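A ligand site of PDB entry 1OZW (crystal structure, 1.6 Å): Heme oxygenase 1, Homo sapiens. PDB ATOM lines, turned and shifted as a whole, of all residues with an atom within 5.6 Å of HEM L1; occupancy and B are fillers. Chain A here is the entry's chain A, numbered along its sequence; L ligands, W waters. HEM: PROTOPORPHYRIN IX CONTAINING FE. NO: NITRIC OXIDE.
NE2 of His 25 is bound to FE of HEM L1 (2.1 Å). OH of Tyr 134 sits at hydrogen-bond distance from O1D of HEM L1 (2.7 Å). O2D of HEM L1 is in salt-bridge range of NH2 of Arg 183 (3.0 Å). The side-chain amino group (NZ) of Lys 18 lies within salt-bridge range of an oxygen (O2A) of HEM L1, 3.5 Å away. O of Gly 139 lies close to O of NO L2 (2.7 Å).
A nitrogen (N) of NO L2 is bound to an iron atom (FE) of HEM L1 (1.7 Å).
OE2 of Glu 29 is in hydrogen-bond range of ND1 of His 25. OE1 of Gln 38 sits close to O of Met 34, at 3.0 Å. The side-chain amide oxygen of Asn 210 is in hydrogen-bond range of the guanidinium group of Arg 136 (2.7 Å). The side-chain hydroxyl (OH) of Tyr 114 sits at hydrogen-bond distance from the side-chain amide nitrogen (ND2) of Asn 210, 3.0 Å away. The backbone carbonyl oxygen (O) of Ala 206 is in hydrogen-bond range of the side-chain amide nitrogen (ND2) of Asn 210 (2.7 Å). The side-chain hydroxyl (OH) of Tyr 114 is in hydrogen-bond range of the guanidinium group (NH1) of Arg 136, at 3.1 Å. The guanidinium group (NE) of Arg 136 lies within salt-bridge range of the side-chain carboxylate (OD2) of Asp 140, at 3.2 Å. OE1 of Gln 38 lies close to O of Glu 29, 2.9 Å away.
Merely in contact with HEM L1: Met 34, Asn 210, Gly 139, Arg 136, Phe 207, Thr 135, Gln 38, Leu 147, Ser 142, Phe 214, Gly 143, Ala 28 and Leu 138. Hydrophobic or aromatic side chains that line HEM L1: His 25, Ala 28, Met 34, Tyr 134, Leu 138, Leu 147, Phe 207 and Phe 214. 17 residues have an atom within 4 Å of HEM L1: Lys 18, His 25, Ala 28, Met 34, Gln 38, Tyr 134, Thr 135, Arg 136, Leu 138, Gly 139, Ser 142, Gly 143, Leu 147, Arg 183, Phe 207, Asn 210 and Phe 214. The nearest printed residue that does not touch HEM L1 is Glu 29 (4.1 Å).
Water W2 lies within hydrogen-bond range of O of Ser 14 (2.7 Å), O1D of HEM L1 (2.7 Å) and NE of Arg 183 (3.1 Å).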
ATOM      1  N   SER A  14       1.109  -7.211 -23.867  1.00  0.00           N
ATOM      2  CA  SER A  14       1.493  -8.586 -24.173  1.00  0.00           C
ATOM      3  C   SER A  14       1.380  -8.874 -25.668  1.00  0.00           C
ATOM      4  O   SER A  14       2.218  -9.567 -26.234  1.00  0.00           O
ATOM      5  CB  SER A  14       0.624  -9.575 -23.380  1.00  0.00           C
ATOM      6  OG  SER A  14      -0.738  -9.476 -23.752  1.00  0.00           O
ATOM      7  N   LEU A  17       4.112  -6.723 -27.570  1.00  0.00           N
ATOM      8  CA  LEU A  17       5.428  -7.345 -27.473  1.00  0.00           C
ATOM      9  C   LEU A  17       5.586  -8.519 -28.440  1.00  0.00           C
ATOM     10  O   LEU A  17       6.597  -8.624 -29.134  1.00  0.00           O
ATOM     11  CB  LEU A  17       5.686  -7.831 -26.047  1.00  0.00           C
ATOM     12  CG  LEU A  17       5.986  -6.748 -25.005  1.00  0.00           C
ATOM     13  CD1 LEU A  17       5.883  -7.339 -23.600  1.00  0.00           C
ATOM     14  CD2 LEU A  17       7.369  -6.179 -25.254  1.00  0.00           C
ATOM     15  N   LYS A  18       4.593  -9.394 -28.478  1.00  0.00           N
ATOM     16  CA  LYS A  18       4.626 -10.555 -29.343  1.00  0.00           C
ATOM     17  C   LYS A  18       4.748 -10.154 -30.815  1.00  0.00           C
ATOM     18  O   LYS A  18       5.534 -10.728 -31.558  1.00  0.00           O
ATOM     19  CB  LYS A  18       3.382 -11.424 -29.138  1.00  0.00           C
ATOM     20  CG  LYS A  18       3.428 -12.742 -29.882  1.00  0.00           C
ATOM     21  CD  LYS A  18       2.233 -13.619 -29.541  1.00  0.00           C
ATOM     22  CE  LYS A  18       2.354 -14.985 -30.200  1.00  0.00           C
ATOM     23  NZ  LYS A  18       1.195 -15.862 -29.867  1.00  0.00           N
ATOM     24  N   HIS A  25      12.505 -12.875 -33.331  1.00  0.00           N
ATOM     25  CA  HIS A  25      12.403 -14.248 -32.837  1.00  0.00           C
ATOM     26  C   HIS A  25      12.796 -15.187 -33.970  1.00  0.00           C
ATOM     27  O   HIS A  25      13.494 -16.182 -33.745  1.00  0.00           O
ATOM     28  CB  HIS A  25      10.970 -14.570 -32.374  1.00  0.00           C
ATOM     29  CG  HIS A  25      10.839 -15.903 -31.695  1.00  0.00           C
ATOM     30  ND1 HIS A  25      10.894 -17.097 -32.388  1.00  0.00           N
ATOM     31  CD2 HIS A  25      10.686 -16.230 -30.390  1.00  0.00           C
ATOM     32  CE1 HIS A  25      10.781 -18.106 -31.530  1.00  0.00           C
ATOM     33  NE2 HIS A  25      10.651 -17.602 -30.313  1.00  0.00           N
ATOM     34  N   ALA A  28      16.372 -15.350 -34.376  1.00  0.00           N
ATOM     35  CA  ALA A  28      16.970 -16.239 -33.385  1.00  0.00           C
ATOM     36  C   ALA A  28      16.860 -17.686 -33.844  1.00  0.00           C
ATOM     37  O   ALA A  28      17.784 -18.475 -33.680  1.00  0.00           O
ATOM     38  CB  ALA A  28      16.284 -16.053 -32.030  1.00  0.00           C
ATOM     39  N   GLU A  29      15.708 -18.038 -34.427  1.00  0.00           N
ATOM     40  CA  GLU A  29      15.496 -19.390 -34.918  1.00  0.00           C
ATOM     41  C   GLU A  29      16.434 -19.682 -36.077  1.00  0.00           C
ATOM     42  O   GLU A  29      16.839 -20.826 -36.288  1.00  0.00           O
ATOM     43  CB  GLU A  29      14.052 -19.570 -35.407  1.00  0.00           C
ATOM     44  CG  GLU A  29      12.991 -19.464 -34.343  1.00  0.00           C
ATOM     45  CD  GLU A  29      11.601 -19.584 -34.930  1.00  0.00           C
ATOM     46  OE1 GLU A  29      11.276 -20.654 -35.494  1.00  0.00           O
ATOM     47  OE2 GLU A  29      10.824 -18.606 -34.831  1.00  0.00           O
ATOM     48  N   MET A  34      21.440 -22.024 -33.449  1.00  0.00           N
ATOM     49  CA  MET A  34      20.103 -22.535 -33.205  1.00  0.00           C
ATOM     50  C   MET A  34      19.603 -23.441 -34.331  1.00  0.00           C
ATOM     51  O   MET A  34      18.802 -24.339 -34.092  1.00  0.00           O
ATOM     52  CB  MET A  34      19.126 -21.386 -32.990  1.00  0.00           C
ATOM     53  CG  MET A  34      19.277 -20.704 -31.636  1.00  0.00           C
ATOM     54  SD  MET A  34      18.850 -21.785 -30.259  1.00  0.00           S
ATOM     55  CE  MET A  34      20.436 -22.361 -29.759  1.00  0.00           C
ATOM     56  N   PHE A  37      21.031 -26.714 -33.487  1.00  0.00           N
ATOM     57  CA  PHE A  37      20.321 -27.240 -32.332  1.00  0.00           C
ATOM     58  C   PHE A  37      19.026 -27.874 -32.798  1.00  0.00           C
ATOM     59  O   PHE A  37      18.720 -29.026 -32.461  1.00  0.00           O
ATOM     60  CB  PHE A  37      20.039 -26.109 -31.336  1.00  0.00           C
ATOM     61  CG  PHE A  37      19.421 -26.569 -30.042  1.00  0.00           C
ATOM     62  CD1 PHE A  37      18.087 -26.976 -29.990  1.00  0.00           C
ATOM     63  CD2 PHE A  37      20.167 -26.597 -28.866  1.00  0.00           C
ATOM     64  CE1 PHE A  37      17.504 -27.392 -28.793  1.00  0.00           C
ATOM     65  CE2 PHE A  37      19.596 -27.002 -27.663  1.00  0.00           C
ATOM     66  CZ  PHE A  37      18.262 -27.402 -27.624  1.00  0.00           C
ATOM     67  N   GLN A  38      18.260 -27.134 -33.584  1.00  0.00           N
ATOM     68  CA  GLN A  38      16.983 -27.614 -34.102  1.00  0.00           C
ATOM     69  C   GLN A  38      17.140 -28.852 -34.983  1.00  0.00           C
ATOM     70  O   GLN A  38      16.304 -29.760 -34.928  1.00  0.00           O
ATOM     71  CB  GLN A  38      16.290 -26.497 -34.881  1.00  0.00           C
ATOM     72  CG  GLN A  38      15.689 -25.435 -33.984  1.00  0.00           C
ATOM     73  CD  GLN A  38      15.306 -24.180 -34.740  1.00  0.00           C
ATOM     74  OE1 GLN A  38      16.161 -23.388 -35.133  1.00  0.00           O
ATOM     75  NE2 GLN A  38      14.005 -23.996 -34.977  1.00  0.00           N
ATOM     76  N   TYR A 114      25.335  -9.191 -22.076  1.00  0.00           N
ATOM     77  CA  TYR A 114      23.939  -9.432 -21.716  1.00  0.00           C
ATOM     78  C   TYR A 114      23.748  -9.100 -20.219  1.00  0.00           C
ATOM     79  O   TYR A 114      22.832  -8.379 -19.842  1.00  0.00           O
ATOM     80  CB  TYR A 114      23.611 -10.911 -21.975  1.00  0.00           C
ATOM     81  CG  TYR A 114      22.139 -11.270 -22.133  1.00  0.00           C
ATOM     82  CD1 TYR A 114      21.131 -10.544 -21.502  1.00  0.00           C
ATOM     83  CD2 TYR A 114      21.767 -12.409 -22.856  1.00  0.00           C
ATOM     84  CE1 TYR A 114      19.798 -10.944 -21.580  1.00  0.00           C
ATOM     85  CE2 TYR A 114      20.445 -12.822 -22.949  1.00  0.00           C
ATOM     86  CZ  TYR A 114      19.456 -12.087 -22.306  1.00  0.00           C
ATOM     87  OH  TYR A 114      18.141 -12.508 -22.378  1.00  0.00           O
ATOM     88  N   TYR A 134       9.938 -10.876 -19.626  1.00  0.00           N
ATOM     89  CA  TYR A 134       9.080 -11.414 -20.672  1.00  0.00           C
ATOM     90  C   TYR A 134       9.874 -12.289 -21.631  1.00  0.00           C
ATOM     91  O   TYR A 134       9.542 -13.453 -21.864  1.00  0.00           O
ATOM     92  CB  TYR A 134       8.431 -10.261 -21.458  1.00  0.00           C
ATOM     93  CG  TYR A 134       7.894 -10.645 -22.835  1.00  0.00           C
ATOM     94  CD1 TYR A 134       6.662 -11.286 -22.976  1.00  0.00           C
ATOM     95  CD2 TYR A 134       8.632 -10.380 -23.998  1.00  0.00           C
ATOM     96  CE1 TYR A 134       6.171 -11.652 -24.251  1.00  0.00           C
ATOM     97  CE2 TYR A 134       8.153 -10.741 -25.255  1.00  0.00           C
ATOM     98  CZ  TYR A 134       6.933 -11.377 -25.378  1.00  0.00           C
ATOM     99  OH  TYR A 134       6.476 -11.736 -26.627  1.00  0.00           O
ATOM    100  N   THR A 135      10.935 -11.716 -22.203  1.00  0.00           N
ATOM    101  CA  THR A 135      11.767 -12.409 -23.169  1.00  0.00           C
ATOM    102  C   THR A 135      12.335 -13.726 -22.619  1.00  0.00           C
ATOM    103  O   THR A 135      12.277 -14.755 -23.285  1.00  0.00           O
ATOM    104  CB  THR A 135      12.937 -11.499 -23.636  1.00  0.00           C
ATOM    105  OG1 THR A 135      12.399 -10.341 -24.287  1.00  0.00           O
ATOM    106  CG2 THR A 135      13.848 -12.229 -24.605  1.00  0.00           C
ATOM    107  N   ARG A 136      12.854 -13.680 -21.396  1.00  0.00           N
ATOM    108  CA  ARG A 136      13.426 -14.880 -20.805  1.00  0.00           C
ATOM    109  C   ARG A 136      12.388 -15.861 -20.272  1.00  0.00           C
ATOM    110  O   ARG A 136      12.291 -16.977 -20.776  1.00  0.00           O
ATOM    111  CB  ARG A 136      14.402 -14.499 -19.686  1.00  0.00           C
ATOM    112  CG  ARG A 136      15.789 -14.118 -20.175  1.00  0.00           C
ATOM    113  CD  ARG A 136      16.746 -15.297 -20.058  1.00  0.00           C
ATOM    114  NE  ARG A 136      16.462 -16.401 -20.977  1.00  0.00           N
ATOM    115  CZ  ARG A 136      16.931 -16.478 -22.214  1.00  0.00           C
ATOM    116  NH1 ARG A 136      17.718 -15.527 -22.687  1.00  0.00           N
ATOM    117  NH2 ARG A 136      16.671 -17.548 -22.960  1.00  0.00           N
ATOM    118  N   LEU A 138       8.786 -16.036 -20.302  1.00  0.00           N
ATOM    119  CA  LEU A 138       7.727 -16.496 -21.182  1.00  0.00           C
ATOM    120  C   LEU A 138       8.323 -17.270 -22.349  1.00  0.00           C
ATOM    121  O   LEU A 138       7.716 -18.194 -22.878  1.00  0.00           O
ATOM    122  CB  LEU A 138       6.866 -15.329 -21.675  1.00  0.00           C
ATOM    123  CG  LEU A 138       5.423 -15.629 -22.080  1.00  0.00           C
ATOM    124  CD1 LEU A 138       4.691 -16.267 -20.917  1.00  0.00           C
ATOM    125  CD2 LEU A 138       4.736 -14.343 -22.503  1.00  0.00           C
ATOM    126  N   GLY A 139       9.538 -16.898 -22.737  1.00  0.00           N
ATOM    127  CA  GLY A 139      10.202 -17.604 -23.825  1.00  0.00           C
ATOM    128  C   GLY A 139      10.590 -19.017 -23.419  1.00  0.00           C
ATOM    129  O   GLY A 139      10.284 -19.969 -24.148  1.00  0.00           O
ATOM    130  N   ASP A 140      11.254 -19.170 -22.279  1.00  0.00           N
ATOM    131  CA  ASP A 140      11.674 -20.500 -21.842  1.00  0.00           C
ATOM    132  C   ASP A 140      10.507 -21.370 -21.411  1.00  0.00           C
ATOM    133  O   ASP A 140      10.577 -22.593 -21.475  1.00  0.00           O
ATOM    134  CB  ASP A 140      12.725 -20.365 -20.718  1.00  0.00           C
ATOM    135  CG  ASP A 140      13.956 -19.597 -21.167  1.00  0.00           C
ATOM    136  OD1 ASP A 140      14.309 -19.687 -22.361  1.00  0.00           O
ATOM    137  OD2 ASP A 140      14.594 -18.914 -20.338  1.00  0.00           O
ATOM    138  N   SER A 142       7.362 -21.075 -22.831  1.00  0.00           N
ATOM    139  CA  SER A 142       6.678 -21.420 -24.077  1.00  0.00           C
ATOM    140  C   SER A 142       7.442 -22.384 -24.984  1.00  0.00           C
ATOM    141  O   SER A 142       6.861 -23.327 -25.531  1.00  0.00           O
ATOM    142  CB  SER A 142       6.360 -20.146 -24.864  1.00  0.00           C
ATOM    143  OG  SER A 142       5.539 -19.278 -24.113  1.00  0.00           O
ATOM    144  N   GLY A 143       8.737 -22.138 -25.168  1.00  0.00           N
ATOM    145  CA  GLY A 143       9.527 -22.993 -26.030  1.00  0.00           C
ATOM    146  C   GLY A 143      10.349 -24.042 -25.307  1.00  0.00           C
ATOM    147  O   GLY A 143      11.106 -24.781 -25.933  1.00  0.00           O
ATOM    148  N   VAL A 146       9.750 -27.857 -26.537  1.00  0.00           N
ATOM    149  CA  VAL A 146      10.387 -28.196 -27.809  1.00  0.00           C
ATOM    150  C   VAL A 146      11.904 -28.210 -27.705  1.00  0.00           C
ATOM    151  O   VAL A 146      12.567 -29.099 -28.229  1.00  0.00           O
ATOM    152  CB  VAL A 146       9.962 -27.212 -28.938  1.00  0.00           C
ATOM    153  CG1 VAL A 146       8.453 -27.249 -29.121  1.00  0.00           C
ATOM    154  CG2 VAL A 146      10.419 -25.795 -28.608  1.00  0.00           C
ATOM    155  N   LEU A 147      12.465 -27.219 -27.009  1.00  0.00           N
ATOM    156  CA  LEU A 147      13.906 -27.121 -26.842  1.00  0.00           C
ATOM    157  C   LEU A 147      14.487 -28.268 -26.029  1.00  0.00           C
ATOM    158  O   LEU A 147      15.604 -28.725 -26.297  1.00  0.00           O
ATOM    159  CB  LEU A 147      14.266 -25.781 -26.187  1.00  0.00           C
ATOM    160  CG  LEU A 147      13.813 -24.530 -26.944  1.00  0.00           C
ATOM    161  CD1 LEU A 147      14.085 -23.293 -26.094  1.00  0.00           C
ATOM    162  CD2 LEU A 147      14.527 -24.444 -28.287  1.00  0.00           C
ATOM    163  N   ARG A 183       0.438 -12.656 -18.770  1.00  0.00           N
ATOM    164  CA  ARG A 183       0.091 -11.673 -19.791  1.00  0.00           C
ATOM    165  C   ARG A 183      -0.876 -10.648 -19.197  1.00  0.00           C
ATOM    166  O   ARG A 183      -0.739  -9.452 -19.424  1.00  0.00           O
ATOM    167  CB  ARG A 183      -0.547 -12.349 -21.009  1.00  0.00           C
ATOM    168  CG  ARG A 183       0.410 -13.234 -21.802  1.00  0.00           C
ATOM    169  CD  ARG A 183      -0.160 -13.523 -23.181  1.00  0.00           C
ATOM    170  NE  ARG A 183       0.726 -14.369 -23.993  1.00  0.00           N
ATOM    171  CZ  ARG A 183       0.782 -15.690 -23.908  1.00  0.00           C
ATOM    172  NH1 ARG A 183       0.009 -16.336 -23.053  1.00  0.00           N
ATOM    173  NH2 ARG A 183       1.612 -16.369 -24.694  1.00  0.00           N
ATOM    174  N   ALA A 206      16.757  -7.422 -26.126  1.00  0.00           N
ATOM    175  CA  ALA A 206      16.979  -8.692 -25.414  1.00  0.00           C
ATOM    176  C   ALA A 206      17.215  -9.801 -26.430  1.00  0.00           C
ATOM    177  O   ALA A 206      18.141 -10.599 -26.271  1.00  0.00           O
ATOM    178  CB  ALA A 206      15.770  -9.024 -24.543  1.00  0.00           C
ATOM    179  N   PHE A 207      16.380  -9.853 -27.463  1.00  0.00           N
ATOM    180  CA  PHE A 207      16.558 -10.875 -28.499  1.00  0.00           C
ATOM    181  C   PHE A 207      17.913 -10.709 -29.169  1.00  0.00           C
ATOM    182  O   PHE A 207      18.608 -11.691 -29.416  1.00  0.00           O
ATOM    183  CB  PHE A 207      15.445 -10.783 -29.560  1.00  0.00           C
ATOM    184  CG  PHE A 207      14.196 -11.533 -29.203  1.00  0.00           C
ATOM    185  CD1 PHE A 207      13.217 -10.944 -28.419  1.00  0.00           C
ATOM    186  CD2 PHE A 207      14.009 -12.844 -29.651  1.00  0.00           C
ATOM    187  CE1 PHE A 207      12.055 -11.652 -28.083  1.00  0.00           C
ATOM    188  CE2 PHE A 207      12.854 -13.548 -29.321  1.00  0.00           C
ATOM    189  CZ  PHE A 207      11.882 -12.955 -28.542  1.00  0.00           C
ATOM    190  N   ASN A 210      20.700 -12.113 -27.218  1.00  0.00           N
ATOM    191  CA  ASN A 210      20.715 -13.574 -27.286  1.00  0.00           C
ATOM    192  C   ASN A 210      21.344 -14.007 -28.602  1.00  0.00           C
ATOM    193  O   ASN A 210      22.140 -14.949 -28.651  1.00  0.00           O
ATOM    194  CB  ASN A 210      19.282 -14.116 -27.211  1.00  0.00           C
ATOM    195  CG  ASN A 210      18.765 -14.211 -25.781  1.00  0.00           C
ATOM    196  OD1 ASN A 210      19.000 -15.193 -25.096  1.00  0.00           O
ATOM    197  ND2 ASN A 210      18.055 -13.186 -25.348  1.00  0.00           N
ATOM    198  N   PHE A 214      24.565 -16.320 -29.324  1.00  0.00           N
ATOM    199  CA  PHE A 214      24.567 -17.521 -30.168  1.00  0.00           C
ATOM    200  C   PHE A 214      25.704 -17.487 -31.158  1.00  0.00           C
ATOM    201  O   PHE A 214      26.374 -18.495 -31.386  1.00  0.00           O
ATOM    202  CB  PHE A 214      23.259 -17.650 -30.956  1.00  0.00           C
ATOM    203  CG  PHE A 214      22.045 -17.906 -30.104  1.00  0.00           C
ATOM    204  CD1 PHE A 214      22.138 -18.610 -28.914  1.00  0.00           C
ATOM    205  CD2 PHE A 214      20.800 -17.454 -30.519  1.00  0.00           C
ATOM    206  CE1 PHE A 214      21.004 -18.875 -28.145  1.00  0.00           C
ATOM    207  CE2 PHE A 214      19.659 -17.712 -29.770  1.00  0.00           C
ATOM    208  CZ  PHE A 214      19.759 -18.417 -28.573  1.00  0.00           C
HETATM  209  CHA HEM L   1       7.593 -18.347 -27.909  1.00  0.00           C
HETATM  210  CHB HEM L   1      10.342 -21.857 -29.891  1.00  0.00           C
HETATM  211  CHC HEM L   1      14.249 -19.007 -29.433  1.00  0.00           C
HETATM  212  CHD HEM L   1      11.633 -15.952 -26.732  1.00  0.00           C
HETATM  213  C1A HEM L   1       7.996 -19.539 -28.536  1.00  0.00           C
HETATM  214  C2A HEM L   1       7.105 -20.653 -28.855  1.00  0.00           C
HETATM  215  C3A HEM L   1       7.895 -21.671 -29.309  1.00  0.00           C
HETATM  216  C4A HEM L   1       9.267 -21.175 -29.319  1.00  0.00           C
HETATM  217  CMA HEM L   1       7.440 -23.051 -29.762  1.00  0.00           C
HETATM  218  CAA HEM L   1       5.564 -20.699 -28.775  1.00  0.00           C
HETATM  219  CBA HEM L   1       4.866 -19.807 -29.795  1.00  0.00           C
HETATM  220  CGA HEM L   1       3.345 -19.975 -29.783  1.00  0.00           C
HETATM  221  O1A HEM L   1       2.871 -21.099 -30.049  1.00  0.00           O
HETATM  222  O2A HEM L   1       2.640 -18.986 -29.508  1.00  0.00           O
HETATM  223  C1B HEM L   1      11.631 -21.330 -30.025  1.00  0.00           C
HETATM  224  C2B HEM L   1      12.688 -21.954 -30.796  1.00  0.00           C
HETATM  225  C3B HEM L   1      13.782 -21.145 -30.691  1.00  0.00           C
HETATM  226  C4B HEM L   1      13.383 -20.014 -29.866  1.00  0.00           C
HETATM  227  CMB HEM L   1      12.569 -23.183 -31.684  1.00  0.00           C
HETATM  228  CAB HEM L   1      15.015 -21.340 -31.329  1.00  0.00           C
HETATM  229  CBB HEM L   1      15.798 -22.558 -31.189  1.00  0.00           C
HETATM  230  C1C HEM L   1      13.871 -17.957 -28.593  1.00  0.00           C
HETATM  231  C2C HEM L   1      14.800 -16.994 -28.018  1.00  0.00           C
HETATM  232  C3C HEM L   1      14.088 -16.195 -27.191  1.00  0.00           C
HETATM  233  C4C HEM L   1      12.708 -16.640 -27.291  1.00  0.00           C
HETATM  234  CMC HEM L   1      16.301 -16.887 -28.287  1.00  0.00           C
HETATM  235  CAC HEM L   1      14.590 -15.175 -26.371  1.00  0.00           C
HETATM  236  CBC HEM L   1      15.576 -15.389 -25.327  1.00  0.00           C
HETATM  237  C1D HEM L   1      10.303 -16.283 -26.926  1.00  0.00           C
HETATM  238  C2D HEM L   1       9.214 -15.509 -26.388  1.00  0.00           C
HETATM  239  C3D HEM L   1       8.083 -16.155 -26.705  1.00  0.00           C
HETATM  240  C4D HEM L   1       8.461 -17.355 -27.469  1.00  0.00           C
HETATM  241  CMD HEM L   1       9.316 -14.261 -25.522  1.00  0.00           C
HETATM  242  CAD HEM L   1       6.709 -15.679 -26.244  1.00  0.00           C
HETATM  243  CBD HEM L   1       5.782 -15.214 -27.356  1.00  0.00           C
HETATM  244  CGD HEM L   1       4.481 -14.652 -26.830  1.00  0.00           C
HETATM  245  O1D HEM L   1       4.472 -13.494 -26.368  1.00  0.00           O
HETATM  246  O2D HEM L   1       3.458 -15.367 -26.884  1.00  0.00           O
HETATM  247  NA  HEM L   1       9.329 -19.872 -28.819  1.00  0.00           N
HETATM  248  NB  HEM L   1      12.054 -20.113 -29.509  1.00  0.00           N
HETATM  249  NC  HEM L   1      12.575 -17.743 -28.118  1.00  0.00           N
HETATM  250  ND  HEM L   1       9.854 -17.413 -27.612  1.00  0.00           N
HETATM  251 FE   HEM L   1      10.941 -18.767 -28.570  1.00  0.00          FE
HETATM  252  N    NO L   2      10.987 -19.648 -27.174  1.00  0.00           N
HETATM  253  O    NO L   2      11.764 -19.979 -26.411  1.00  0.00           O
HETATM  254  O   HOH W   1      13.431 -17.251 -23.703  1.00  0.00           O
HETATM  255  O   HOH W   2       2.302 -12.146 -25.482  1.00  0.00           O
